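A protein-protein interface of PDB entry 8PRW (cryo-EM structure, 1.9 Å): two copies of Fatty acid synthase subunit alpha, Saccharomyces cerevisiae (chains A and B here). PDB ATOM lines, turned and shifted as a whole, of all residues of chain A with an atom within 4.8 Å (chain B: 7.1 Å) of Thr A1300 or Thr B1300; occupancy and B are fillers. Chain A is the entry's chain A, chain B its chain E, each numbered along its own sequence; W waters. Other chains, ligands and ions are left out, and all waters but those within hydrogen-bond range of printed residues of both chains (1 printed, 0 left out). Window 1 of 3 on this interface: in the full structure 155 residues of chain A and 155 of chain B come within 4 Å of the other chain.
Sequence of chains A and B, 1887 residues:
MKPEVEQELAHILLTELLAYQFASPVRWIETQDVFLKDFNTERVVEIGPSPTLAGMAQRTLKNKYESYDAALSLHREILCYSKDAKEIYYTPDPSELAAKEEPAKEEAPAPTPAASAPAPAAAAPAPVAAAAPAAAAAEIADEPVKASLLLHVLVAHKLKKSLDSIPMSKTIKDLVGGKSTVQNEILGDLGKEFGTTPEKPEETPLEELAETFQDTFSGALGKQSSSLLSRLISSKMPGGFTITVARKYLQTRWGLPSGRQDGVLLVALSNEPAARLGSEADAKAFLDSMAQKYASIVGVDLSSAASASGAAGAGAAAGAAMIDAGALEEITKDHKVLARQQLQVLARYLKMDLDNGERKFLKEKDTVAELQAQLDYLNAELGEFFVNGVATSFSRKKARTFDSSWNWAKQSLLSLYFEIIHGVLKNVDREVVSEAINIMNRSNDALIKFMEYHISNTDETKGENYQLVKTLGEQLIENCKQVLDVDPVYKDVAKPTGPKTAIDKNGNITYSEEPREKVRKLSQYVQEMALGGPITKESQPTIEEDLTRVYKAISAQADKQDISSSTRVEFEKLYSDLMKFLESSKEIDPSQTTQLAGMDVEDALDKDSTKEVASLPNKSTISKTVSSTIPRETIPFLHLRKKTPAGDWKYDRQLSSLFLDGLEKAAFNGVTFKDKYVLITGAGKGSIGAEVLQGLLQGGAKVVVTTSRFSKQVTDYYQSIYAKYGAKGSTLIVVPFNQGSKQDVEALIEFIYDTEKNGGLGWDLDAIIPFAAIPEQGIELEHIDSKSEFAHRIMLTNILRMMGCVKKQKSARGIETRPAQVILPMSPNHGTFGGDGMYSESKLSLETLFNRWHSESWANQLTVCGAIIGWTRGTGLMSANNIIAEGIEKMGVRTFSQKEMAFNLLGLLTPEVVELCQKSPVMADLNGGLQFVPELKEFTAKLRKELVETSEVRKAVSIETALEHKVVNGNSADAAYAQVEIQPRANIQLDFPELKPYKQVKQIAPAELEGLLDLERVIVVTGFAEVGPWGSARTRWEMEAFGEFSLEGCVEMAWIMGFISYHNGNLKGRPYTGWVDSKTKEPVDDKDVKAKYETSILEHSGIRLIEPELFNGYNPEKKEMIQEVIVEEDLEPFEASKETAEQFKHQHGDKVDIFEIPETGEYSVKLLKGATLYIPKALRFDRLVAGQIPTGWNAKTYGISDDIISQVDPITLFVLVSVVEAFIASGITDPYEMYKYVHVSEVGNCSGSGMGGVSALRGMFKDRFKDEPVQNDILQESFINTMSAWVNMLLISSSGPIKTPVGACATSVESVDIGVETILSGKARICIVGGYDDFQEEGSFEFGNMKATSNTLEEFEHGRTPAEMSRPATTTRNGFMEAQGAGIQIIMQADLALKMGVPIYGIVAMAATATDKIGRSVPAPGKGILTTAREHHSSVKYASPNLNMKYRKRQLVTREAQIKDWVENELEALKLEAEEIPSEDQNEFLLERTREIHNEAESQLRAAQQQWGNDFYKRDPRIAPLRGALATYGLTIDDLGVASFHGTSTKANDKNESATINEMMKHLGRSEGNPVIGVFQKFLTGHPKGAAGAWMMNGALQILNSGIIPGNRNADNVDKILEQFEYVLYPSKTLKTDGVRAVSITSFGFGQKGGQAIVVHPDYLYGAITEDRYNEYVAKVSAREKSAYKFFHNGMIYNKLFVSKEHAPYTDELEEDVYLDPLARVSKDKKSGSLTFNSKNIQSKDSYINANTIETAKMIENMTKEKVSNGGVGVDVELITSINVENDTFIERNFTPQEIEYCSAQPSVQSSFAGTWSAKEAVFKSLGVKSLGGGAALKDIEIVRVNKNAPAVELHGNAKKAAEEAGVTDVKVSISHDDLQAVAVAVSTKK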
ATOM      1  N   SER A1247      17.293 -28.437 -20.727  1.00  0.00           N
ATOM      2  CA  SER A1247      18.273 -28.700 -19.673  1.00  0.00           C
ATOM      3  C   SER A1247      17.714 -28.232 -18.358  1.00  0.00           C
ATOM      4  O   SER A1247      16.803 -27.383 -18.346  1.00  0.00           O
ATOM      5  CB  SER A1247      19.603 -28.024 -19.947  1.00  0.00           C
ATOM      6  OG  SER A1247      19.431 -26.656 -19.857  1.00  0.00           O
ATOM      7  N   GLY A1248      18.209 -28.808 -17.301  1.00  0.00           N
ATOM      8  CA  GLY A1248      17.752 -28.435 -15.973  1.00  0.00           C
ATOM      9  C   GLY A1248      18.735 -28.586 -14.869  1.00  0.00           C
ATOM     10  O   GLY A1248      19.927 -28.796 -15.064  1.00  0.00           O
ATOM     11  N   ILE A1280      15.585 -22.210 -11.249  1.00  0.00           N
ATOM     12  CA  ILE A1280      16.199 -23.338 -11.995  1.00  0.00           C
ATOM     13  C   ILE A1280      16.146 -23.066 -13.476  1.00  0.00           C
ATOM     14  O   ILE A1280      17.125 -23.374 -14.194  1.00  0.00           O
ATOM     15  CB  ILE A1280      15.594 -24.666 -11.591  1.00  0.00           C
ATOM     16  CG1 ILE A1280      16.148 -25.011 -10.217  1.00  0.00           C
ATOM     17  CG2 ILE A1280      15.888 -25.729 -12.637  1.00  0.00           C
ATOM     18  CD1 ILE A1280      15.403 -26.070  -9.533  1.00  0.00           C
ATOM     19  N   ASN A1281      15.131 -22.339 -13.922  1.00  0.00           N
ATOM     20  CA  ASN A1281      15.008 -22.033 -15.350  1.00  0.00           C
ATOM     21  C   ASN A1281      15.723 -20.778 -15.788  1.00  0.00           C
ATOM     22  O   ASN A1281      15.780 -20.553 -16.986  1.00  0.00           O
ATOM     23  CB  ASN A1281      13.553 -21.945 -15.771  1.00  0.00           C
ATOM     24  CG  ASN A1281      12.835 -20.831 -15.047  1.00  0.00           C
ATOM     25  OD1 ASN A1281      12.696 -20.881 -13.834  1.00  0.00           O
ATOM     26  ND2 ASN A1281      12.322 -19.875 -15.798  1.00  0.00           N
ATOM     27  N   SER A1284      18.748 -21.423 -18.362  1.00  0.00           N
ATOM     28  CA  SER A1284      18.269 -21.578 -19.746  1.00  0.00           C
ATOM     29  C   SER A1284      17.829 -20.245 -20.331  1.00  0.00           C
ATOM     30  O   SER A1284      17.986 -20.021 -21.521  1.00  0.00           O
ATOM     31  CB  SER A1284      17.131 -22.594 -19.847  1.00  0.00           C
ATOM     32  OG  SER A1284      17.623 -23.873 -19.554  1.00  0.00           O
ATOM     33  N   ILE A1298      10.872 -24.607 -24.177  1.00  0.00           N
ATOM     34  CA  ILE A1298      11.704 -24.405 -22.990  1.00  0.00           C
ATOM     35  C   ILE A1298      11.035 -25.218 -21.898  1.00  0.00           C
ATOM     36  O   ILE A1298       9.991 -24.777 -21.357  1.00  0.00           O
ATOM     37  CB  ILE A1298      11.834 -22.926 -22.693  1.00  0.00           C
ATOM     38  CG1 ILE A1298      12.568 -22.721 -21.373  1.00  0.00           C
ATOM     39  CG2 ILE A1298      10.487 -22.205 -22.683  1.00  0.00           C
ATOM     40  CD1 ILE A1298      13.972 -22.876 -21.453  1.00  0.00           C
ATOM     41  N   LYS A1299      11.576 -26.384 -21.625  1.00  0.00           N
ATOM     42  CA  LYS A1299      10.995 -27.294 -20.638  1.00  0.00           C
ATOM     43  C   LYS A1299      12.127 -27.602 -19.697  1.00  0.00           C
ATOM     44  O   LYS A1299      13.036 -28.287 -20.125  1.00  0.00           O
ATOM     45  CB  LYS A1299      10.476 -28.534 -21.353  1.00  0.00           C
ATOM     46  CG  LYS A1299       9.223 -28.298 -22.171  1.00  0.00           C
ATOM     47  CD  LYS A1299       8.973 -29.384 -23.122  1.00  0.00           C
ATOM     48  CE  LYS A1299       7.589 -29.338 -23.692  1.00  0.00           C
ATOM     49  NZ  LYS A1299       7.420 -30.427 -24.682  1.00  0.00           N
ATOM     50  N   THR A1300      12.125 -27.007 -18.539  1.00  0.00           N
ATOM     51  CA  THR A1300      13.212 -27.096 -17.583  1.00  0.00           C
ATOM     52  C   THR A1300      12.834 -28.161 -16.564  1.00  0.00           C
ATOM     53  O   THR A1300      11.988 -27.951 -15.720  1.00  0.00           O
ATOM     54  CB  THR A1300      13.481 -25.768 -16.943  1.00  0.00           C
ATOM     55  OG1 THR A1300      13.620 -24.811 -17.977  1.00  0.00           O
ATOM     56  CG2 THR A1300      14.686 -25.836 -16.045  1.00  0.00           C
ATOM     57  N   PRO A1301      13.499 -29.331 -16.573  1.00  0.00           N
ATOM     58  CA  PRO A1301      13.274 -30.332 -15.568  1.00  0.00           C
ATOM     59  C   PRO A1301      14.057 -30.081 -14.288  1.00  0.00           C
ATOM     60  O   PRO A1301      15.090 -29.476 -14.241  1.00  0.00           O
ATOM     61  CB  PRO A1301      13.755 -31.622 -16.191  1.00  0.00           C
ATOM     62  CG  PRO A1301      14.864 -31.163 -17.090  1.00  0.00           C
ATOM     63  CD  PRO A1301      14.417 -29.790 -17.606  1.00  0.00           C
ATOM     64  N   VAL A1302      13.481 -30.605 -13.238  1.00  0.00           N
ATOM     65  CA  VAL A1302      14.120 -30.708 -11.931  1.00  0.00           C
ATOM     66  C   VAL A1302      13.985 -32.169 -11.518  1.00  0.00           C
ATOM     67  O   VAL A1302      12.850 -32.676 -11.404  1.00  0.00           O
ATOM     68  CB  VAL A1302      13.449 -29.794 -10.912  1.00  0.00           C
ATOM     69  CG1 VAL A1302      14.210 -29.863  -9.594  1.00  0.00           C
ATOM     70  CG2 VAL A1302      13.581 -28.420 -11.445  1.00  0.00           C
ATOM     71  N   GLU A1310      16.335 -37.092 -17.208  1.00  0.00           N
ATOM     72  CA  GLU A1310      15.011 -36.474 -17.446  1.00  0.00           C
ATOM     73  C   GLU A1310      15.087 -35.438 -18.570  1.00  0.00           C
ATOM     74  O   GLU A1310      14.198 -35.371 -19.389  1.00  0.00           O
ATOM     75  CB  GLU A1310      14.560 -35.864 -16.120  1.00  0.00           C
ATOM     76  CG  GLU A1310      13.208 -35.224 -16.200  1.00  0.00           C
ATOM     77  CD  GLU A1310      12.703 -34.621 -14.871  1.00  0.00           C
ATOM     78  OE1 GLU A1310      13.205 -35.021 -13.790  1.00  0.00           O
ATOM     79  OE2 GLU A1310      11.820 -33.719 -14.921  1.00  0.00           O
ATOM     80  N   LYS A1649      13.204 -40.432  -8.612  1.00  0.00           N
ATOM     81  CA  LYS A1649      13.519 -40.061  -9.990  1.00  0.00           C
ATOM     82  C   LYS A1649      14.452 -41.148 -10.536  1.00  0.00           C
ATOM     83  O   LYS A1649      15.654 -41.062 -10.307  1.00  0.00           O
ATOM     84  CB  LYS A1649      14.181 -38.714 -10.026  1.00  0.00           C
ATOM     85  CG  LYS A1649      13.268 -37.534  -9.822  1.00  0.00           C
ATOM     86  CD  LYS A1649      12.748 -36.978 -11.102  1.00  0.00           C
ATOM     87  CE  LYS A1649      11.766 -35.856 -10.792  1.00  0.00           C
ATOM     88  NZ  LYS A1649      11.369 -35.130 -12.014  1.00  0.00           N
ATOM     89  N   ASN B1245       3.513 -38.272 -13.526  1.00  0.00           N
ATOM     90  CA  ASN B1245       3.338 -37.001 -12.838  1.00  0.00           C
ATOM     91  C   ASN B1245       4.219 -35.995 -13.548  1.00  0.00           C
ATOM     92  O   ASN B1245       5.462 -36.135 -13.461  1.00  0.00           O
ATOM     93  CB  ASN B1245       3.551 -37.112 -11.335  1.00  0.00           C
ATOM     94  CG  ASN B1245       3.044 -35.866 -10.620  1.00  0.00           C
ATOM     95  OD1 ASN B1245       2.914 -34.771 -11.184  1.00  0.00           O
ATOM     96  ND2 ASN B1245       2.667 -36.015  -9.365  1.00  0.00           N
ATOM     97  N   CYS B1246       3.605 -34.984 -14.168  1.00  0.00           N
ATOM     98  CA  CYS B1246       4.381 -33.927 -14.865  1.00  0.00           C
ATOM     99  C   CYS B1246       4.118 -32.562 -14.221  1.00  0.00           C
ATOM    100  O   CYS B1246       4.381 -31.554 -14.890  1.00  0.00           O
ATOM    101  CB  CYS B1246       4.033 -33.877 -16.347  1.00  0.00           C
ATOM    102  SG  CYS B1246       4.383 -35.429 -17.215  1.00  0.00           S
ATOM    103  N   SER B1247       3.634 -32.534 -12.974  1.00  0.00           N
ATOM    104  CA  SER B1247       3.339 -31.273 -12.294  1.00  0.00           C
ATOM    105  C   SER B1247       4.623 -30.686 -11.776  1.00  0.00           C
ATOM    106  O   SER B1247       5.609 -31.426 -11.598  1.00  0.00           O
ATOM    107  CB  SER B1247       2.349 -31.454 -11.158  1.00  0.00           C
ATOM    108  OG  SER B1247       2.951 -32.195 -10.160  1.00  0.00           O
ATOM    109  N   GLY B1248       4.616 -29.396 -11.594  1.00  0.00           N
ATOM    110  CA  GLY B1248       5.797 -28.716 -11.090  1.00  0.00           C
ATOM    111  C   GLY B1248       5.561 -27.477 -10.304  1.00  0.00           C
ATOM    112  O   GLY B1248       4.452 -27.147  -9.901  1.00  0.00           O
ATOM    113  N   SER B1249       6.631 -26.767 -10.094  1.00  0.00           N
ATOM    114  CA  SER B1249       6.621 -25.584  -9.228  1.00  0.00           C
ATOM    115  C   SER B1249       7.633 -24.606  -9.753  1.00  0.00           C
ATOM    116  O   SER B1249       8.573 -25.043 -10.399  1.00  0.00           O
ATOM    117  CB  SER B1249       6.839 -25.990  -7.874  1.00  0.00           C
ATOM    118  OG  SER B1249       6.918 -24.902  -6.983  1.00  0.00           O
ATOM    119  N   PHE B1279      13.047 -29.630  -2.459  1.00  0.00           N
ATOM    120  CA  PHE B1279      13.213 -29.881  -3.903  1.00  0.00           C
ATOM    121  C   PHE B1279      11.879 -29.759  -4.620  1.00  0.00           C
ATOM    122  O   PHE B1279      10.882 -30.253  -4.127  1.00  0.00           O
ATOM    123  CB  PHE B1279      13.728 -31.258  -4.234  1.00  0.00           C
ATOM    124  CG  PHE B1279      15.087 -31.591  -3.717  1.00  0.00           C
ATOM    125  CD1 PHE B1279      16.031 -30.606  -3.513  1.00  0.00           C
ATOM    126  CD2 PHE B1279      15.364 -32.889  -3.349  1.00  0.00           C
ATOM    127  CE1 PHE B1279      17.281 -30.943  -3.015  1.00  0.00           C
ATOM    128  CE2 PHE B1279      16.615 -33.225  -2.850  1.00  0.00           C
ATOM    129  CZ  PHE B1279      17.566 -32.248  -2.724  1.00  0.00           C
ATOM    130  N   ILE B1280      11.921 -29.174  -5.794  1.00  0.00           N
ATOM    131  CA  ILE B1280      10.695 -28.938  -6.598  1.00  0.00           C
ATOM    132  C   ILE B1280      10.034 -30.251  -6.926  1.00  0.00           C
ATOM    133  O   ILE B1280       8.785 -30.337  -6.892  1.00  0.00           O
ATOM    134  CB  ILE B1280      10.982 -28.074  -7.809  1.00  0.00           C
ATOM    135  CG1 ILE B1280      11.169 -26.650  -7.307  1.00  0.00           C
ATOM    136  CG2 ILE B1280       9.869 -28.204  -8.836  1.00  0.00           C
ATOM    137  CD1 ILE B1280      11.797 -25.760  -8.287  1.00  0.00           C
ATOM    138  N   ASN B1281      10.821 -31.311  -7.056  1.00  0.00           N
ATOM    139  CA  ASN B1281      10.254 -32.622  -7.378  1.00  0.00           C
ATOM    140  C   ASN B1281       9.840 -33.438  -6.178  1.00  0.00           C
ATOM    141  O   ASN B1281       9.227 -34.474  -6.386  1.00  0.00           O
ATOM    142  CB  ASN B1281      11.207 -33.442  -8.228  1.00  0.00           C
ATOM    143  CG  ASN B1281      12.498 -33.718  -7.498  1.00  0.00           C
ATOM    144  OD1 ASN B1281      13.237 -32.794  -7.192  1.00  0.00           O
ATOM    145  ND2 ASN B1281      12.798 -34.987  -7.289  1.00  0.00           N
ATOM    146  N   THR B1282      10.036 -32.952  -4.985  1.00  0.00           N
ATOM    147  CA  THR B1282       9.668 -33.721  -3.782  1.00  0.00           C
ATOM    148  C   THR B1282       8.161 -33.760  -3.653  1.00  0.00           C
ATOM    149  O   THR B1282       7.674 -34.726  -3.073  1.00  0.00           O
ATOM    150  CB  THR B1282      10.348 -33.154  -2.525  1.00  0.00           C
ATOM    151  OG1 THR B1282      11.731 -33.553  -2.616  1.00  0.00           O
ATOM    152  CG2 THR B1282       9.783 -33.729  -1.252  1.00  0.00           C
ATOM    153  N   MET B1283       7.429 -32.723  -4.073  1.00  0.00           N
ATOM    154  CA  MET B1283       5.947 -32.769  -3.952  1.00  0.00           C
ATOM    155  C   MET B1283       5.394 -33.936  -4.741  1.00  0.00           C
ATOM    156  O   MET B1283       4.555 -34.663  -4.200  1.00  0.00           O
ATOM    157  CB  MET B1283       5.273 -31.478  -4.425  1.00  0.00           C
ATOM    158  CG  MET B1283       5.649 -30.271  -3.629  1.00  0.00           C
ATOM    159  SD  MET B1283       7.248 -29.486  -4.031  1.00  0.00           S
ATOM    160  CE  MET B1283       8.068 -29.592  -2.435  1.00  0.00           C
ATOM    161  N   SER B1284       5.885 -34.149  -5.958  1.00  0.00           N
ATOM    162  CA  SER B1284       5.481 -35.281  -6.810  1.00  0.00           C
ATOM    163  C   SER B1284       5.926 -36.606  -6.213  1.00  0.00           C
ATOM    164  O   SER B1284       5.238 -37.604  -6.366  1.00  0.00           O
ATOM    165  CB  SER B1284       6.016 -35.143  -8.235  1.00  0.00           C
ATOM    166  OG  SER B1284       5.391 -34.057  -8.862  1.00  0.00           O
ATOM    167  N   ALA B1285       7.071 -36.618  -5.577  1.00  0.00           N
ATOM    168  CA  ALA B1285       7.530 -37.837  -4.913  1.00  0.00           C
ATOM    169  C   ALA B1285       6.517 -38.176  -3.799  1.00  0.00           C
ATOM    170  O   ALA B1285       6.085 -39.299  -3.719  1.00  0.00           O
ATOM    171  CB  ALA B1285       8.906 -37.595  -4.358  1.00  0.00           C
ATOM    172  N   ILE B1298       8.048 -39.292 -14.609  1.00  0.00           N
ATOM    173  CA  ILE B1298       8.082 -38.230 -13.602  1.00  0.00           C
ATOM    174  C   ILE B1298       8.942 -37.139 -14.210  1.00  0.00           C
ATOM    175  O   ILE B1298      10.189 -37.284 -14.237  1.00  0.00           O
ATOM    176  CB  ILE B1298       8.589 -38.781 -12.287  1.00  0.00           C
ATOM    177  CG1 ILE B1298       8.773 -37.649 -11.283  1.00  0.00           C
ATOM    178  CG2 ILE B1298       9.879 -39.585 -12.439  1.00  0.00           C
ATOM    179  CD1 ILE B1298       7.573 -37.196 -10.684  1.00  0.00           C
ATOM    180  N   LYS B1299       8.303 -36.115 -14.731  1.00  0.00           N
ATOM    181  CA  LYS B1299       9.008 -35.025 -15.405  1.00  0.00           C
ATOM    182  C   LYS B1299       8.519 -33.779 -14.717  1.00  0.00           C
ATOM    183  O   LYS B1299       7.363 -33.454 -14.911  1.00  0.00           O
ATOM    184  CB  LYS B1299       8.660 -35.050 -16.886  1.00  0.00           C
ATOM    185  CG  LYS B1299       9.288 -36.197 -17.650  1.00  0.00           C
ATOM    186  CD  LYS B1299       8.647 -36.407 -18.952  1.00  0.00           C
ATOM    187  CE  LYS B1299       9.453 -37.296 -19.848  1.00  0.00           C
ATOM    188  NZ  LYS B1299       8.727 -37.510 -21.122  1.00  0.00           N
ATOM    189  N   THR B1300       9.318 -33.214 -13.858  1.00  0.00           N
ATOM    190  CA  THR B1300       8.940 -32.092 -13.020  1.00  0.00           C
ATOM    191  C   THR B1300       9.453 -30.829 -13.694  1.00  0.00           C
ATOM    192  O   THR B1300      10.635 -30.550 -13.690  1.00  0.00           O
ATOM    193  CB  THR B1300       9.473 -32.251 -11.628  1.00  0.00           C
ATOM    194  OG1 THR B1300       9.106 -33.540 -11.171  1.00  0.00           O
ATOM    195  CG2 THR B1300       8.977 -31.151 -10.731  1.00  0.00           C
ATOM    196  N   PRO B1301       8.566 -29.984 -14.249  1.00  0.00           N
ATOM    197  CA  PRO B1301       8.971 -28.719 -14.797  1.00  0.00           C
ATOM    198  C   PRO B1301       9.109 -27.629 -13.746  1.00  0.00           C
ATOM    199  O   PRO B1301       8.502 -27.612 -12.712  1.00  0.00           O
ATOM    200  CB  PRO B1301       7.866 -28.339 -15.755  1.00  0.00           C
ATOM    201  CG  PRO B1301       6.652 -28.950 -15.120  1.00  0.00           C
ATOM    202  CD  PRO B1301       7.152 -30.247 -14.473  1.00  0.00           C
ATOM    203  N   VAL B1302       9.963 -26.701 -14.095  1.00  0.00           N
ATOM    204  CA  VAL B1302      10.120 -25.437 -13.385  1.00  0.00           C
ATOM    205  C   VAL B1302       9.999 -24.349 -14.445  1.00  0.00           C
ATOM    206  O   VAL B1302      10.801 -24.326 -15.402  1.00  0.00           O
ATOM    207  CB  VAL B1302      11.470 -25.360 -12.681  1.00  0.00           C
ATOM    208  CG1 VAL B1302      11.548 -24.070 -11.877  1.00  0.00           C
ATOM    209  CG2 VAL B1302      11.504 -26.495 -11.732  1.00  0.00           C
ATOM    210  N   GLY B1303       8.992 -23.546 -14.334  1.00  0.00           N
ATOM    211  CA  GLY B1303       8.713 -22.553 -15.362  1.00  0.00           C
ATOM    212  C   GLY B1303       8.238 -21.275 -14.793  1.00  0.00           C
ATOM    213  O   GLY B1303       7.567 -20.604 -15.525  1.00  0.00           O
ATOM    214  N   THR B1307       4.744 -22.431 -15.193  1.00  0.00           N
ATOM    215  CA  THR B1307       4.984 -23.841 -14.847  1.00  0.00           C
ATOM    216  C   THR B1307       3.815 -24.734 -15.207  1.00  0.00           C
ATOM    217  O   THR B1307       4.026 -25.875 -15.718  1.00  0.00           O
ATOM    218  CB  THR B1307       5.343 -23.944 -13.368  1.00  0.00           C
ATOM    219  OG1 THR B1307       6.490 -23.152 -13.106  1.00  0.00           O
ATOM    220  CG2 THR B1307       5.554 -25.368 -12.994  1.00  0.00           C
ATOM    221  N   GLU B1310       3.615 -25.305 -18.969  1.00  0.00           N
ATOM    222  CA  GLU B1310       4.723 -26.236 -19.275  1.00  0.00           C
ATOM    223  C   GLU B1310       4.383 -27.656 -18.821  1.00  0.00           C
ATOM    224  O   GLU B1310       4.672 -28.599 -19.524  1.00  0.00           O
ATOM    225  CB  GLU B1310       5.971 -25.686 -18.586  1.00  0.00           C
ATOM    226  CG  GLU B1310       7.192 -26.515 -18.836  1.00  0.00           C
ATOM    227  CD  GLU B1310       8.481 -25.975 -18.179  1.00  0.00           C
ATOM    228  OE1 GLU B1310       8.536 -24.764 -17.849  1.00  0.00           O
ATOM    229  OE2 GLU B1310       9.428 -26.785 -17.967  1.00  0.00           O
ATOM    230  N   ILE B1314       4.257 -30.922 -21.233  1.00  0.00           N
ATOM    231  CA  ILE B1314       5.031 -32.156 -20.913  1.00  0.00           C
ATOM    232  C   ILE B1314       4.097 -33.331 -20.786  1.00  0.00           C
ATOM    233  O   ILE B1314       4.390 -34.362 -21.388  1.00  0.00           O
ATOM    234  CB  ILE B1314       5.885 -31.954 -19.664  1.00  0.00           C
ATOM    235  CG1 ILE B1314       6.978 -30.935 -19.969  1.00  0.00           C
ATOM    236  CG2 ILE B1314       6.470 -33.275 -19.214  1.00  0.00           C
ATOM    237  CD1 ILE B1314       7.658 -30.472 -18.744  1.00  0.00           C
ATOM    238  N   TYR B1332       2.196 -25.491  -8.514  1.00  0.00           N
ATOM    239  CA  TYR B1332       2.088 -25.167  -7.106  1.00  0.00           C
ATOM    240  C   TYR B1332       3.145 -24.193  -6.783  1.00  0.00           C
ATOM    241  O   TYR B1332       4.249 -24.277  -7.314  1.00  0.00           O
ATOM    242  CB  TYR B1332       2.071 -26.402  -6.225  1.00  0.00           C
ATOM    243  CG  TYR B1332       2.791 -27.582  -6.795  1.00  0.00           C
ATOM    244  CD1 TYR B1332       2.108 -28.471  -7.600  1.00  0.00           C
ATOM    245  CD2 TYR B1332       4.102 -27.847  -6.499  1.00  0.00           C
ATOM    246  CE1 TYR B1332       2.756 -29.543  -8.188  1.00  0.00           C
ATOM    247  CE2 TYR B1332       4.766 -28.946  -7.054  1.00  0.00           C
ATOM    248  CZ  TYR B1332       4.063 -29.827  -7.854  1.00  0.00           C
ATOM    249  OH  TYR B1332       4.614 -30.927  -8.469  1.00  0.00           O
ATOM    250  N   LYS B1649       9.634 -17.756 -20.253  1.00  0.00           N
ATOM    251  CA  LYS B1649       8.766 -18.931 -20.274  1.00  0.00           C
ATOM    252  C   LYS B1649       7.407 -18.467 -20.808  1.00  0.00           C
ATOM    253  O   LYS B1649       6.606 -17.968 -20.023  1.00  0.00           O
ATOM    254  CB  LYS B1649       8.635 -19.504 -18.892  1.00  0.00           C
ATOM    255  CG  LYS B1649       9.826 -20.279 -18.393  1.00  0.00           C
ATOM    256  CD  LYS B1649       9.728 -21.738 -18.681  1.00  0.00           C
ATOM    257  CE  LYS B1649      11.011 -22.420 -18.227  1.00  0.00           C
ATOM    258  NZ  LYS B1649      10.898 -23.890 -18.297  1.00  0.00           N
HETATM  259  O   HOH W   1      10.337 -30.671 -17.170  1.00  0.00           O
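Lys A1299 touches Glu B1310, and with the chains exchanged Glu A1310 touches Lys B1299. Thr A1300 touches Pro B1301, and with the chains exchanged Pro A1301 touches Thr B1300. Val A1302 touches its own counterpart, Val B1302. 12 positions are printed for both chains.
Water W1 lies within hydrogen-bond range of O of Thr B1300 (3.5 Å) and O of Thr A1300 (3.5 Å).
The backbone carbonyl oxygen (O) of Val A1302 lies within hydrogen-bond range of the side-chain amino group (NZ) of Lys A1649 (2.9 Å). N of Ser B1249 is in hydrogen-bond range of O of Pro B1301 (3.3 Å).
Hydrophobic or aromatic side chains of chain A that line the printed part of chain B: Ile A1280, Ile A1298 and Val A1302. Printed residues of chain B that touch a printed residue of chain A: Ile B1280, Asn B1281, Ile B1298, Lys B1299, Thr B1300, Pro B1301, Val B1302, Glu B1310 and Lys B1649. Hydrophobic or aromatic side chains of chain B within 4 Å of the printed part of chain A: Ile B1280, Ile B1298 and Val B1302. Among the printed residues, 21 pairs touch across the chains. Among the printed residues, no Asp or Glu carboxylate lies within 4 Å of a Lys or Arg side-chain nitrogen of the other chain.
Among the printed residues, merely in contact across the chains: Ile A1280 with Ile B1280 (3.8 Å), Asn A1281 with Val B1302 (3.7 Å), Asn A1281 with Lys B1649 (3.6 Å), Ile A1298 with Glu B1310 (3.7 Å), Lys A1299 with Glu B1310 (3.1 Å), Thr A1300 with Thr B1300 (3.6 Å), Thr A1300 with Pro B1301 (3.2 Å), Pro A1301 with Thr B1300 (3.2 Å), Val A1302 with Asn B1281 (3.7 Å), Val A1302 with Val B1302 (2.8 Å), Glu A1310 with Ile B1298 (3.7 Å), Glu A1310 with Lys B1299 (3.1 Å) and Lys A1649 with Asn B1281 (3.6 Å).
Thr A1300 touches five residues of chain B. Printed residues of chain B within 4 Å of Glu A1310: Ile B1298 (3.7 Å), Lys B1299 (3.1 Å) and Thr B1300 (2.8 Å). Of the printed residues of chain A, Lys B1299 touches Glu A1310 (3.1 Å). Of chain A, only Thr A1300 (3.6 Å), Pro A1301 (3.2 Å), Val A1302 (2.9 Å), Glu A1310 (2.8 Å) and Lys A1649 (2.9 Å) come within 4 Å of Thr B1300. Printed residues of chain A within 4 Å of Pro B1301: Thr A1300 (3.2 Å). The nearest residue of chain B that does not touch Thr A1300 is Gly B1303 (5.5 Å). The nearest printed residue of chain A that does not touch Thr B1300 is Lys A1299 (6.9 Å).
OE2 of Glu B1310 lies within hydrogen-bond range of N of Thr A1300, 2.8 Å away. The side-chain amino group (NZ) of Lys B1649 is in hydrogen-bond range of the side-chain hydroxyl (OG1) of Thr A1300 (2.9 Å). The side-chain amino group (NZ) of Lys A1649 sits at hydrogen-bond distance from the backbone carbonyl oxygen (O) of Ile B1298 (3.3 Å). OG1 of Thr B1300 sits at hydrogen-bond distance from NZ of Lys A1649. The backbone NH of Val B1302 sits at hydrogen-bond distance from the backbone carbonyl oxygen of Thr A1300 (2.9 Å). The backbone NH (N) of Thr B1300 is in hydrogen-bond range of the side-chain carboxylate (OE2) of Glu A1310 (2.8 Å). The backbone NH (N) of Val A1302 is in hydrogen-bond range of the backbone carbonyl oxygen (O) of Thr B1300, at 2.9 Å. The side-chain amino group (NZ) of Lys B1649 lies within hydrogen-bond range of the backbone carbonyl oxygen (O) of Ile A1298 (3.3 Å).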
